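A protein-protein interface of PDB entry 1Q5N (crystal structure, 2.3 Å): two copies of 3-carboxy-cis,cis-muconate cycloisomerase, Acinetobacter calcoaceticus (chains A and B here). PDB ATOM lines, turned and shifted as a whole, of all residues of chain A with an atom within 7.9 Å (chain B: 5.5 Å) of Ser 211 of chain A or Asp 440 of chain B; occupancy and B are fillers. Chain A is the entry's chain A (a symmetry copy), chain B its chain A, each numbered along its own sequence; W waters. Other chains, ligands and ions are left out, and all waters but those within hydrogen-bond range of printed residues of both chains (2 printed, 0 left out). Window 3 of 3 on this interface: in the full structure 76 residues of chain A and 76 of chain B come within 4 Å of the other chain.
Ser 211 of chain A touches two residues of chain B.
Asp 440 of chain B touches one residue of chain A.
Printed residues of chain B within 4 Å of Gln 207 of chain A: Asn 437.
Printed residues of chain A within 4 Å of Ile 438 of chain B: Ser 202.
Of the printed residues of chain B, Ser 202 of chain A touches Asn 437 (3.0 Å) and Ile 438 (3.5 Å).
Printed residues of chain A within 4 Å of Asn 437 of chain B: Ser 202, Leu 203, Gln 207, Gly 210 and Ser 211.
Of the printed residues of chain B, Cys 228 of chain A touches Gln 441.
The nearest printed residue of chain B that does not touch Ser 211 of chain A is Gln 441 of chain B (5.5 Å).
The nearest printed residue of chain B that does not touch Gln 207 of chain A is Ile 438 of chain B (6.5 Å).
The side-chain amide nitrogen (NE2) of Gln 441 of chain B lies within hydrogen-bond range of the side-chain amide oxygen (OD1) of Asn 437 of chain B, at 2.8 Å.
Of the 9 printed residues of chain B, 5 touch a printed residue of chain A.
Hydrophobic or aromatic side chains of chain B that line the printed part of chain A: Ile 438 and Ala 444.
Among the printed residues, 10 pairs touch across the chains.
Among the printed residues, no Asp or Glu carboxylate lies within 4 Å of a Lys or Arg side-chain nitrogen of the other chain.
No position is printed for both chains.
Of the 10 pairs that touch across the chains among the printed residues, none has its exchanged pair printed and touching as well.
Among the printed residues, merely in contact across the chains: Cys 228 of chain A with Gln 441 of chain B, Ser 202 of chain A with Ile 438 of chain B, Ala 227 of chain A with Gln 441 of chain B, Gly 210 of chain A with Asn 437 of chain B, Ala 227 of chain A with Ala 444 of chain B, Leu 203 of chain A with Asn 437 of chain B and Gln 207 of chain A with Asn 437 of chain B.
The side-chain amide nitrogen (ND2) of Asn 437 of chain B is in hydrogen-bond range of the side-chain hydroxyl (OG) of Ser 211 of chain A (3.0 Å).
The backbone NH of Asn 437 of chain B is in hydrogen-bond range of the backbone carbonyl oxygen of Ser 202 of chain A (3.0 Å).
The side-chain hydroxyl of Ser 211 of chain A is in hydrogen-bond range of the side-chain carboxylate of Asp 440 of chain B (2.5 Å).
Water W1 lies within hydrogen-bond range of O of Gln 207 of chain A (2.8 Å), N of Gly 210 of chain A (2.9 Å), O of Leu 203 of chain A (3.1 Å) and N of Asn 437 of chain B (3.5 Å).
Water W2 lies within hydrogen-bond range of the backbone carbonyl oxygen (O) of Asp 208 of chain A, the side-chain carboxylate (OD2) of Asp 440 of chain B, the side-chain hydroxyl (OG) of Ser 211 of chain A and the backbone NH (N) of Gly 210 of chain A.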
ATOM      1  N   VAL A  44     -20.059 -10.403 -15.253  1.00  0.00           N
ATOM      2  CA  VAL A  44     -20.829 -10.981 -14.146  1.00  0.00           C
ATOM      3  C   VAL A  44     -21.353  -9.904 -13.190  1.00  0.00           C
ATOM      4  O   VAL A  44     -21.840 -10.209 -12.098  1.00  0.00           O
ATOM      5  CB  VAL A  44     -20.001 -11.988 -13.307  1.00  0.00           C
ATOM      6  CG1 VAL A  44     -19.601 -13.165 -14.155  1.00  0.00           C
ATOM      7  CG2 VAL A  44     -18.779 -11.299 -12.703  1.00  0.00           C
ATOM      8  N   LEU A 196      -5.897 -16.581 -10.245  1.00  0.00           N
ATOM      9  CA  LEU A 196      -6.605 -15.385  -9.745  1.00  0.00           C
ATOM     10  C   LEU A 196      -7.096 -15.700  -8.322  1.00  0.00           C
ATOM     11  O   LEU A 196      -8.081 -16.424  -8.118  1.00  0.00           O
ATOM     12  CB  LEU A 196      -7.781 -15.000 -10.648  1.00  0.00           C
ATOM     13  CG  LEU A 196      -8.529 -13.737 -10.161  1.00  0.00           C
ATOM     14  CD1 LEU A 196      -7.635 -12.518 -10.307  1.00  0.00           C
ATOM     15  CD2 LEU A 196      -9.811 -13.518 -10.980  1.00  0.00           C
ATOM     16  N   SER A 202      -7.590 -15.693  -1.272  1.00  0.00           N
ATOM     17  CA  SER A 202      -8.983 -15.861  -0.797  1.00  0.00           C
ATOM     18  C   SER A 202      -9.991 -15.014  -1.592  1.00  0.00           C
ATOM     19  O   SER A 202     -11.177 -15.144  -1.387  1.00  0.00           O
ATOM     20  CB  SER A 202      -9.086 -15.460   0.671  1.00  0.00           C
ATOM     21  OG  SER A 202      -8.892 -14.059   0.746  1.00  0.00           O
ATOM     22  N   LEU A 203      -9.500 -14.178  -2.505  1.00  0.00           N
ATOM     23  CA  LEU A 203     -10.340 -13.273  -3.283  1.00  0.00           C
ATOM     24  C   LEU A 203     -11.249 -12.492  -2.327  1.00  0.00           C
ATOM     25  O   LEU A 203     -12.377 -12.167  -2.675  1.00  0.00           O
ATOM     26  CB  LEU A 203     -11.179 -14.043  -4.330  1.00  0.00           C
ATOM     27  CG  LEU A 203     -10.357 -14.671  -5.499  1.00  0.00           C
ATOM     28  CD1 LEU A 203     -11.224 -15.558  -6.431  1.00  0.00           C
ATOM     29  CD2 LEU A 203      -9.688 -13.553  -6.305  1.00  0.00           C
ATOM     30  N   LEU A 206     -13.457  -9.472  -3.453  1.00  0.00           N
ATOM     31  CA  LEU A 206     -14.556  -9.742  -4.373  1.00  0.00           C
ATOM     32  C   LEU A 206     -15.734 -10.354  -3.599  1.00  0.00           C
ATOM     33  O   LEU A 206     -16.745 -10.729  -4.184  1.00  0.00           O
ATOM     34  CB  LEU A 206     -14.099 -10.702  -5.486  1.00  0.00           C
ATOM     35  CG  LEU A 206     -13.112 -10.097  -6.495  1.00  0.00           C
ATOM     36  CD1 LEU A 206     -12.761 -11.119  -7.546  1.00  0.00           C
ATOM     37  CD2 LEU A 206     -13.724  -8.870  -7.152  1.00  0.00           C
ATOM     38  N   GLN A 207     -15.559 -10.501  -2.287  1.00  0.00           N
ATOM     39  CA  GLN A 207     -16.573 -11.038  -1.385  1.00  0.00           C
ATOM     40  C   GLN A 207     -17.267 -12.355  -1.686  1.00  0.00           C
ATOM     41  O   GLN A 207     -16.745 -13.402  -1.349  1.00  0.00           O
ATOM     42  CB  GLN A 207     -17.576  -9.917  -1.105  1.00  0.00           C
ATOM     43  CG  GLN A 207     -16.807  -8.832  -0.319  1.00  0.00           C
ATOM     44  CD  GLN A 207     -17.494  -7.502  -0.167  1.00  0.00           C
ATOM     45  OE1 GLN A 207     -17.811  -6.820  -1.162  1.00  0.00           O
ATOM     46  NE2 GLN A 207     -17.702  -7.094   1.093  1.00  0.00           N
ATOM     47  N   ASP A 208     -18.456 -12.346  -2.263  1.00  0.00           N
ATOM     48  CA  ASP A 208     -19.063 -13.642  -2.561  1.00  0.00           C
ATOM     49  C   ASP A 208     -19.177 -13.914  -4.060  1.00  0.00           C
ATOM     50  O   ASP A 208     -19.806 -14.868  -4.490  1.00  0.00           O
ATOM     51  CB  ASP A 208     -20.419 -13.794  -1.849  1.00  0.00           C
ATOM     52  CG  ASP A 208     -21.429 -12.712  -2.228  1.00  0.00           C
ATOM     53  OD1 ASP A 208     -21.051 -11.675  -2.835  1.00  0.00           O
ATOM     54  OD2 ASP A 208     -22.624 -12.905  -1.896  1.00  0.00           O
ATOM     55  N   GLN A 209     -18.504 -13.086  -4.839  1.00  0.00           N
ATOM     56  CA  GLN A 209     -18.469 -13.175  -6.295  1.00  0.00           C
ATOM     57  C   GLN A 209     -17.179 -13.845  -6.775  1.00  0.00           C
ATOM     58  O   GLN A 209     -16.945 -13.963  -7.981  1.00  0.00           O
ATOM     59  CB  GLN A 209     -18.473 -11.763  -6.884  1.00  0.00           C
ATOM     60  CG  GLN A 209     -19.637 -10.923  -6.427  1.00  0.00           C
ATOM     61  CD  GLN A 209     -20.935 -11.519  -6.905  1.00  0.00           C
ATOM     62  OE1 GLN A 209     -21.377 -11.255  -8.034  1.00  0.00           O
ATOM     63  NE2 GLN A 209     -21.544 -12.363  -6.068  1.00  0.00           N
ATOM     64  N   GLY A 210     -16.333 -14.254  -5.838  1.00  0.00           N
ATOM     65  CA  GLY A 210     -15.062 -14.835  -6.230  1.00  0.00           C
ATOM     66  C   GLY A 210     -15.049 -15.979  -7.239  1.00  0.00           C
ATOM     67  O   GLY A 210     -14.374 -15.882  -8.294  1.00  0.00           O
ATOM     68  N   SER A 211     -15.751 -17.067  -6.909  1.00  0.00           N
ATOM     69  CA  SER A 211     -15.779 -18.234  -7.783  1.00  0.00           C
ATOM     70  C   SER A 211     -16.362 -17.916  -9.173  1.00  0.00           C
ATOM     71  O   SER A 211     -15.865 -18.389 -10.184  1.00  0.00           O
ATOM     72  CB  SER A 211     -16.560 -19.338  -7.125  1.00  0.00           C
ATOM     73  OG  SER A 211     -16.244 -19.423  -5.750  1.00  0.00           O
ATOM     74  N   ILE A 212     -17.393 -17.083  -9.209  1.00  0.00           N
ATOM     75  CA  ILE A 212     -18.030 -16.671 -10.458  1.00  0.00           C
ATOM     76  C   ILE A 212     -16.995 -15.909 -11.308  1.00  0.00           C
ATOM     77  O   ILE A 212     -16.861 -16.149 -12.526  1.00  0.00           O
ATOM     78  CB  ILE A 212     -19.242 -15.740 -10.130  1.00  0.00           C
ATOM     79  CG1 ILE A 212     -20.256 -16.498  -9.256  1.00  0.00           C
ATOM     80  CG2 ILE A 212     -19.766 -15.113 -11.346  1.00  0.00           C
ATOM     81  CD1 ILE A 212     -19.846 -16.499  -7.626  1.00  0.00           C
ATOM     82  N   VAL A 213     -16.257 -14.986 -10.693  1.00  0.00           N
ATOM     83  CA  VAL A 213     -15.273 -14.245 -11.466  1.00  0.00           C
ATOM     84  C   VAL A 213     -14.078 -15.094 -11.994  1.00  0.00           C
ATOM     85  O   VAL A 213     -13.619 -14.880 -13.112  1.00  0.00           O
ATOM     86  CB  VAL A 213     -14.714 -13.069 -10.685  1.00  0.00           C
ATOM     87  CG1 VAL A 213     -13.595 -12.418 -11.485  1.00  0.00           C
ATOM     88  CG2 VAL A 213     -15.815 -12.041 -10.438  1.00  0.00           C
ATOM     89  N   VAL A 214     -13.597 -16.068 -11.222  1.00  0.00           N
ATOM     90  CA  VAL A 214     -12.460 -16.887 -11.652  1.00  0.00           C
ATOM     91  C   VAL A 214     -12.886 -17.704 -12.852  1.00  0.00           C
ATOM     92  O   VAL A 214     -12.139 -17.848 -13.833  1.00  0.00           O
ATOM     93  CB  VAL A 214     -11.979 -17.862 -10.530  1.00  0.00           C
ATOM     94  CG1 VAL A 214     -10.750 -18.657 -10.992  1.00  0.00           C
ATOM     95  CG2 VAL A 214     -11.605 -17.069  -9.313  1.00  0.00           C
ATOM     96  N   GLU A 215     -14.096 -18.237 -12.785  1.00  0.00           N
ATOM     97  CA  GLU A 215     -14.605 -19.038 -13.870  1.00  0.00           C
ATOM     98  C   GLU A 215     -14.639 -18.263 -15.193  1.00  0.00           C
ATOM     99  O   GLU A 215     -14.181 -18.756 -16.229  1.00  0.00           O
ATOM    100  CB  GLU A 215     -15.976 -19.542 -13.485  1.00  0.00           C
ATOM    101  CG  GLU A 215     -16.733 -20.212 -14.587  1.00  0.00           C
ATOM    102  CD  GLU A 215     -18.113 -20.586 -14.100  1.00  0.00           C
ATOM    103  OE1 GLU A 215     -18.854 -19.656 -13.661  1.00  0.00           O
ATOM    104  OE2 GLU A 215     -18.438 -21.798 -14.128  1.00  0.00           O
ATOM    105  N   ALA A 216     -15.140 -17.038 -15.148  1.00  0.00           N
ATOM    106  CA  ALA A 216     -15.226 -16.225 -16.349  1.00  0.00           C
ATOM    107  C   ALA A 216     -13.861 -15.680 -16.770  1.00  0.00           C
ATOM    108  O   ALA A 216     -13.642 -15.358 -17.935  1.00  0.00           O
ATOM    109  CB  ALA A 216     -16.211 -15.060 -16.135  1.00  0.00           C
ATOM    110  N   TYR A 217     -12.947 -15.528 -15.824  1.00  0.00           N
ATOM    111  CA  TYR A 217     -11.612 -15.041 -16.166  1.00  0.00           C
ATOM    112  C   TYR A 217     -10.880 -16.171 -16.927  1.00  0.00           C
ATOM    113  O   TYR A 217     -10.271 -15.946 -17.953  1.00  0.00           O
ATOM    114  CB  TYR A 217     -10.893 -14.653 -14.871  1.00  0.00           C
ATOM    115  CG  TYR A 217      -9.424 -14.259 -14.989  1.00  0.00           C
ATOM    116  CD1 TYR A 217      -9.031 -13.131 -15.700  1.00  0.00           C
ATOM    117  CD2 TYR A 217      -8.443 -14.977 -14.290  1.00  0.00           C
ATOM    118  CE1 TYR A 217      -7.695 -12.718 -15.702  1.00  0.00           C
ATOM    119  CE2 TYR A 217      -7.118 -14.581 -14.288  1.00  0.00           C
ATOM    120  CZ  TYR A 217      -6.748 -13.451 -14.985  1.00  0.00           C
ATOM    121  OH  TYR A 217      -5.438 -13.044 -14.926  1.00  0.00           O
ATOM    122  N   GLN A 225      -9.332 -23.821 -15.126  1.00  0.00           N
ATOM    123  CA  GLN A 225      -9.614 -23.173 -13.863  1.00  0.00           C
ATOM    124  C   GLN A 225      -9.120 -24.178 -12.822  1.00  0.00           C
ATOM    125  O   GLN A 225      -9.143 -25.358 -13.089  1.00  0.00           O
ATOM    126  CB  GLN A 225     -11.126 -22.963 -13.746  1.00  0.00           C
ATOM    127  CG  GLN A 225     -11.576 -22.305 -12.470  1.00  0.00           C
ATOM    128  CD  GLN A 225     -13.121 -22.218 -12.349  1.00  0.00           C
ATOM    129  OE1 GLN A 225     -13.631 -21.785 -11.295  1.00  0.00           O
ATOM    130  NE2 GLN A 225     -13.861 -22.618 -13.419  1.00  0.00           N
ATOM    131  N   ALA A 227      -9.192 -25.701  -8.696  1.00  0.00           N
ATOM    132  CA  ALA A 227     -10.045 -25.764  -7.531  1.00  0.00           C
ATOM    133  C   ALA A 227      -9.615 -24.709  -6.485  1.00  0.00           C
ATOM    134  O   ALA A 227     -10.450 -24.040  -5.888  1.00  0.00           O
ATOM    135  CB  ALA A 227      -9.992 -27.195  -6.914  1.00  0.00           C
ATOM    136  N   CYS A 228      -8.325 -24.571  -6.227  1.00  0.00           N
ATOM    137  CA  CYS A 228      -7.913 -23.561  -5.259  1.00  0.00           C
ATOM    138  C   CYS A 228      -6.718 -22.725  -5.779  1.00  0.00           C
ATOM    139  O   CYS A 228      -6.048 -23.110  -6.735  1.00  0.00           O
ATOM    140  CB  CYS A 228      -7.605 -24.225  -3.900  1.00  0.00           C
ATOM    141  SG  CYS A 228      -6.372 -25.485  -4.075  1.00  0.00           S
ATOM    142  N   ASN B 437     -13.956 -16.232  -1.097  1.00  0.00           N
ATOM    143  CA  ASN B 437     -14.527 -17.514  -1.472  1.00  0.00           C
ATOM    144  C   ASN B 437     -13.718 -18.702  -0.965  1.00  0.00           C
ATOM    145  O   ASN B 437     -13.673 -19.740  -1.616  1.00  0.00           O
ATOM    146  CB  ASN B 437     -14.699 -17.608  -2.997  1.00  0.00           C
ATOM    147  CG  ASN B 437     -13.389 -17.985  -3.713  1.00  0.00           C
ATOM    148  OD1 ASN B 437     -12.280 -17.682  -3.239  1.00  0.00           O
ATOM    149  ND2 ASN B 437     -13.522 -18.619  -4.867  1.00  0.00           N
ATOM    150  N   ILE B 438     -13.100 -18.585   0.211  1.00  0.00           N
ATOM    151  CA  ILE B 438     -12.331 -19.722   0.729  1.00  0.00           C
ATOM    152  C   ILE B 438     -13.140 -21.024   0.914  1.00  0.00           C
ATOM    153  O   ILE B 438     -12.619 -22.108   0.704  1.00  0.00           O
ATOM    154  CB  ILE B 438     -11.617 -19.355   2.058  1.00  0.00           C
ATOM    155  CG1 ILE B 438     -10.332 -18.587   1.758  1.00  0.00           C
ATOM    156  CG2 ILE B 438     -11.325 -20.584   2.859  1.00  0.00           C
ATOM    157  CD1 ILE B 438      -9.611 -18.185   2.992  1.00  0.00           C
ATOM    158  N   GLN B 439     -14.411 -20.919   1.314  1.00  0.00           N
ATOM    159  CA  GLN B 439     -15.243 -22.109   1.527  1.00  0.00           C
ATOM    160  C   GLN B 439     -15.573 -22.771   0.202  1.00  0.00           C
ATOM    161  O   GLN B 439     -15.601 -23.997   0.136  1.00  0.00           O
ATOM    162  CB  GLN B 439     -16.512 -21.750   2.343  1.00  0.00           C
ATOM    163  CG  GLN B 439     -16.130 -21.205   3.767  1.00  0.00           C
ATOM    164  CD  GLN B 439     -15.186 -22.136   4.496  1.00  0.00           C
ATOM    165  OE1 GLN B 439     -15.252 -23.344   4.315  1.00  0.00           O
ATOM    166  NE2 GLN B 439     -14.309 -21.592   5.340  1.00  0.00           N
ATOM    167  N   ASP B 440     -15.783 -21.979  -0.856  1.00  0.00           N
ATOM    168  CA  ASP B 440     -16.020 -22.557  -2.185  1.00  0.00           C
ATOM    169  C   ASP B 440     -14.762 -23.346  -2.603  1.00  0.00           C
ATOM    170  O   ASP B 440     -14.864 -24.462  -3.175  1.00  0.00           O
ATOM    171  CB  ASP B 440     -16.256 -21.474  -3.272  1.00  0.00           C
ATOM    172  CG  ASP B 440     -17.599 -20.751  -3.141  1.00  0.00           C
ATOM    173  OD1 ASP B 440     -18.447 -21.187  -2.324  1.00  0.00           O
ATOM    174  OD2 ASP B 440     -17.809 -19.739  -3.858  1.00  0.00           O
ATOM    175  N   GLN B 441     -13.567 -22.781  -2.333  1.00  0.00           N
ATOM    176  CA  GLN B 441     -12.317 -23.470  -2.716  1.00  0.00           C
ATOM    177  C   GLN B 441     -12.160 -24.756  -1.934  1.00  0.00           C
ATOM    178  O   GLN B 441     -11.805 -25.795  -2.521  1.00  0.00           O
ATOM    179  CB  GLN B 441     -11.090 -22.575  -2.526  1.00  0.00           C
ATOM    180  CG  GLN B 441     -10.993 -21.407  -3.549  1.00  0.00           C
ATOM    181  CD  GLN B 441      -9.771 -20.522  -3.277  1.00  0.00           C
ATOM    182  OE1 GLN B 441      -8.632 -21.010  -3.243  1.00  0.00           O
ATOM    183  NE2 GLN B 441     -10.003 -19.224  -3.073  1.00  0.00           N
ATOM    184  N   ILE B 442     -12.437 -24.719  -0.627  1.00  0.00           N
ATOM    185  CA  ILE B 442     -12.312 -25.948   0.123  1.00  0.00           C
ATOM    186  C   ILE B 442     -13.337 -26.994  -0.407  1.00  0.00           C
ATOM    187  O   ILE B 442     -13.000 -28.172  -0.547  1.00  0.00           O
ATOM    188  CB  ILE B 442     -12.502 -25.696   1.635  1.00  0.00           C
ATOM    189  CG1 ILE B 442     -11.356 -24.778   2.129  1.00  0.00           C
ATOM    190  CG2 ILE B 442     -12.611 -27.047   2.392  1.00  0.00           C
ATOM    191  CD1 ILE B 442     -11.369 -24.447   3.641  1.00  0.00           C
ATOM    192  N   ASP B 443     -14.572 -26.576  -0.715  1.00  0.00           N
ATOM    193  CA  ASP B 443     -15.568 -27.526  -1.226  1.00  0.00           C
ATOM    194  C   ASP B 443     -15.107 -28.093  -2.578  1.00  0.00           C
ATOM    195  O   ASP B 443     -15.310 -29.277  -2.867  1.00  0.00           O
ATOM    196  CB  ASP B 443     -16.955 -26.873  -1.447  1.00  0.00           C
ATOM    197  CG  ASP B 443     -17.680 -26.557  -0.147  1.00  0.00           C
ATOM    198  OD1 ASP B 443     -17.501 -27.291   0.853  1.00  0.00           O
ATOM    199  OD2 ASP B 443     -18.450 -25.564  -0.145  1.00  0.00           O
ATOM    200  N   ALA B 444     -14.565 -27.214  -3.424  1.00  0.00           N
ATOM    201  CA  ALA B 444     -14.089 -27.625  -4.732  1.00  0.00           C
ATOM    202  C   ALA B 444     -13.022 -28.718  -4.572  1.00  0.00           C
ATOM    203  O   ALA B 444     -13.098 -29.725  -5.295  1.00  0.00           O
ATOM    204  CB  ALA B 444     -13.554 -26.419  -5.524  1.00  0.00           C
ATOM    205  N   VAL B 445     -12.070 -28.598  -3.622  1.00  0.00           N
ATOM    206  CA  VAL B 445     -11.113 -29.688  -3.528  1.00  0.00           C
ATOM    207  C   VAL B 445     -11.674 -30.937  -2.892  1.00  0.00           C
ATOM    208  O   VAL B 445     -11.192 -32.022  -3.194  1.00  0.00           O
ATOM    209  CB  VAL B 445      -9.719 -29.327  -2.868  1.00  0.00           C
ATOM    210  CG1 VAL B 445      -9.508 -27.858  -2.818  1.00  0.00           C
ATOM    211  CG2 VAL B 445      -9.528 -30.052  -1.597  1.00  0.00           C
HETATM  212  O   HOH W   1     -14.898 -13.797  -3.353  1.00  0.00           O
HETATM  213  O   HOH W   2     -17.974 -16.979  -4.522  1.00  0.00           O
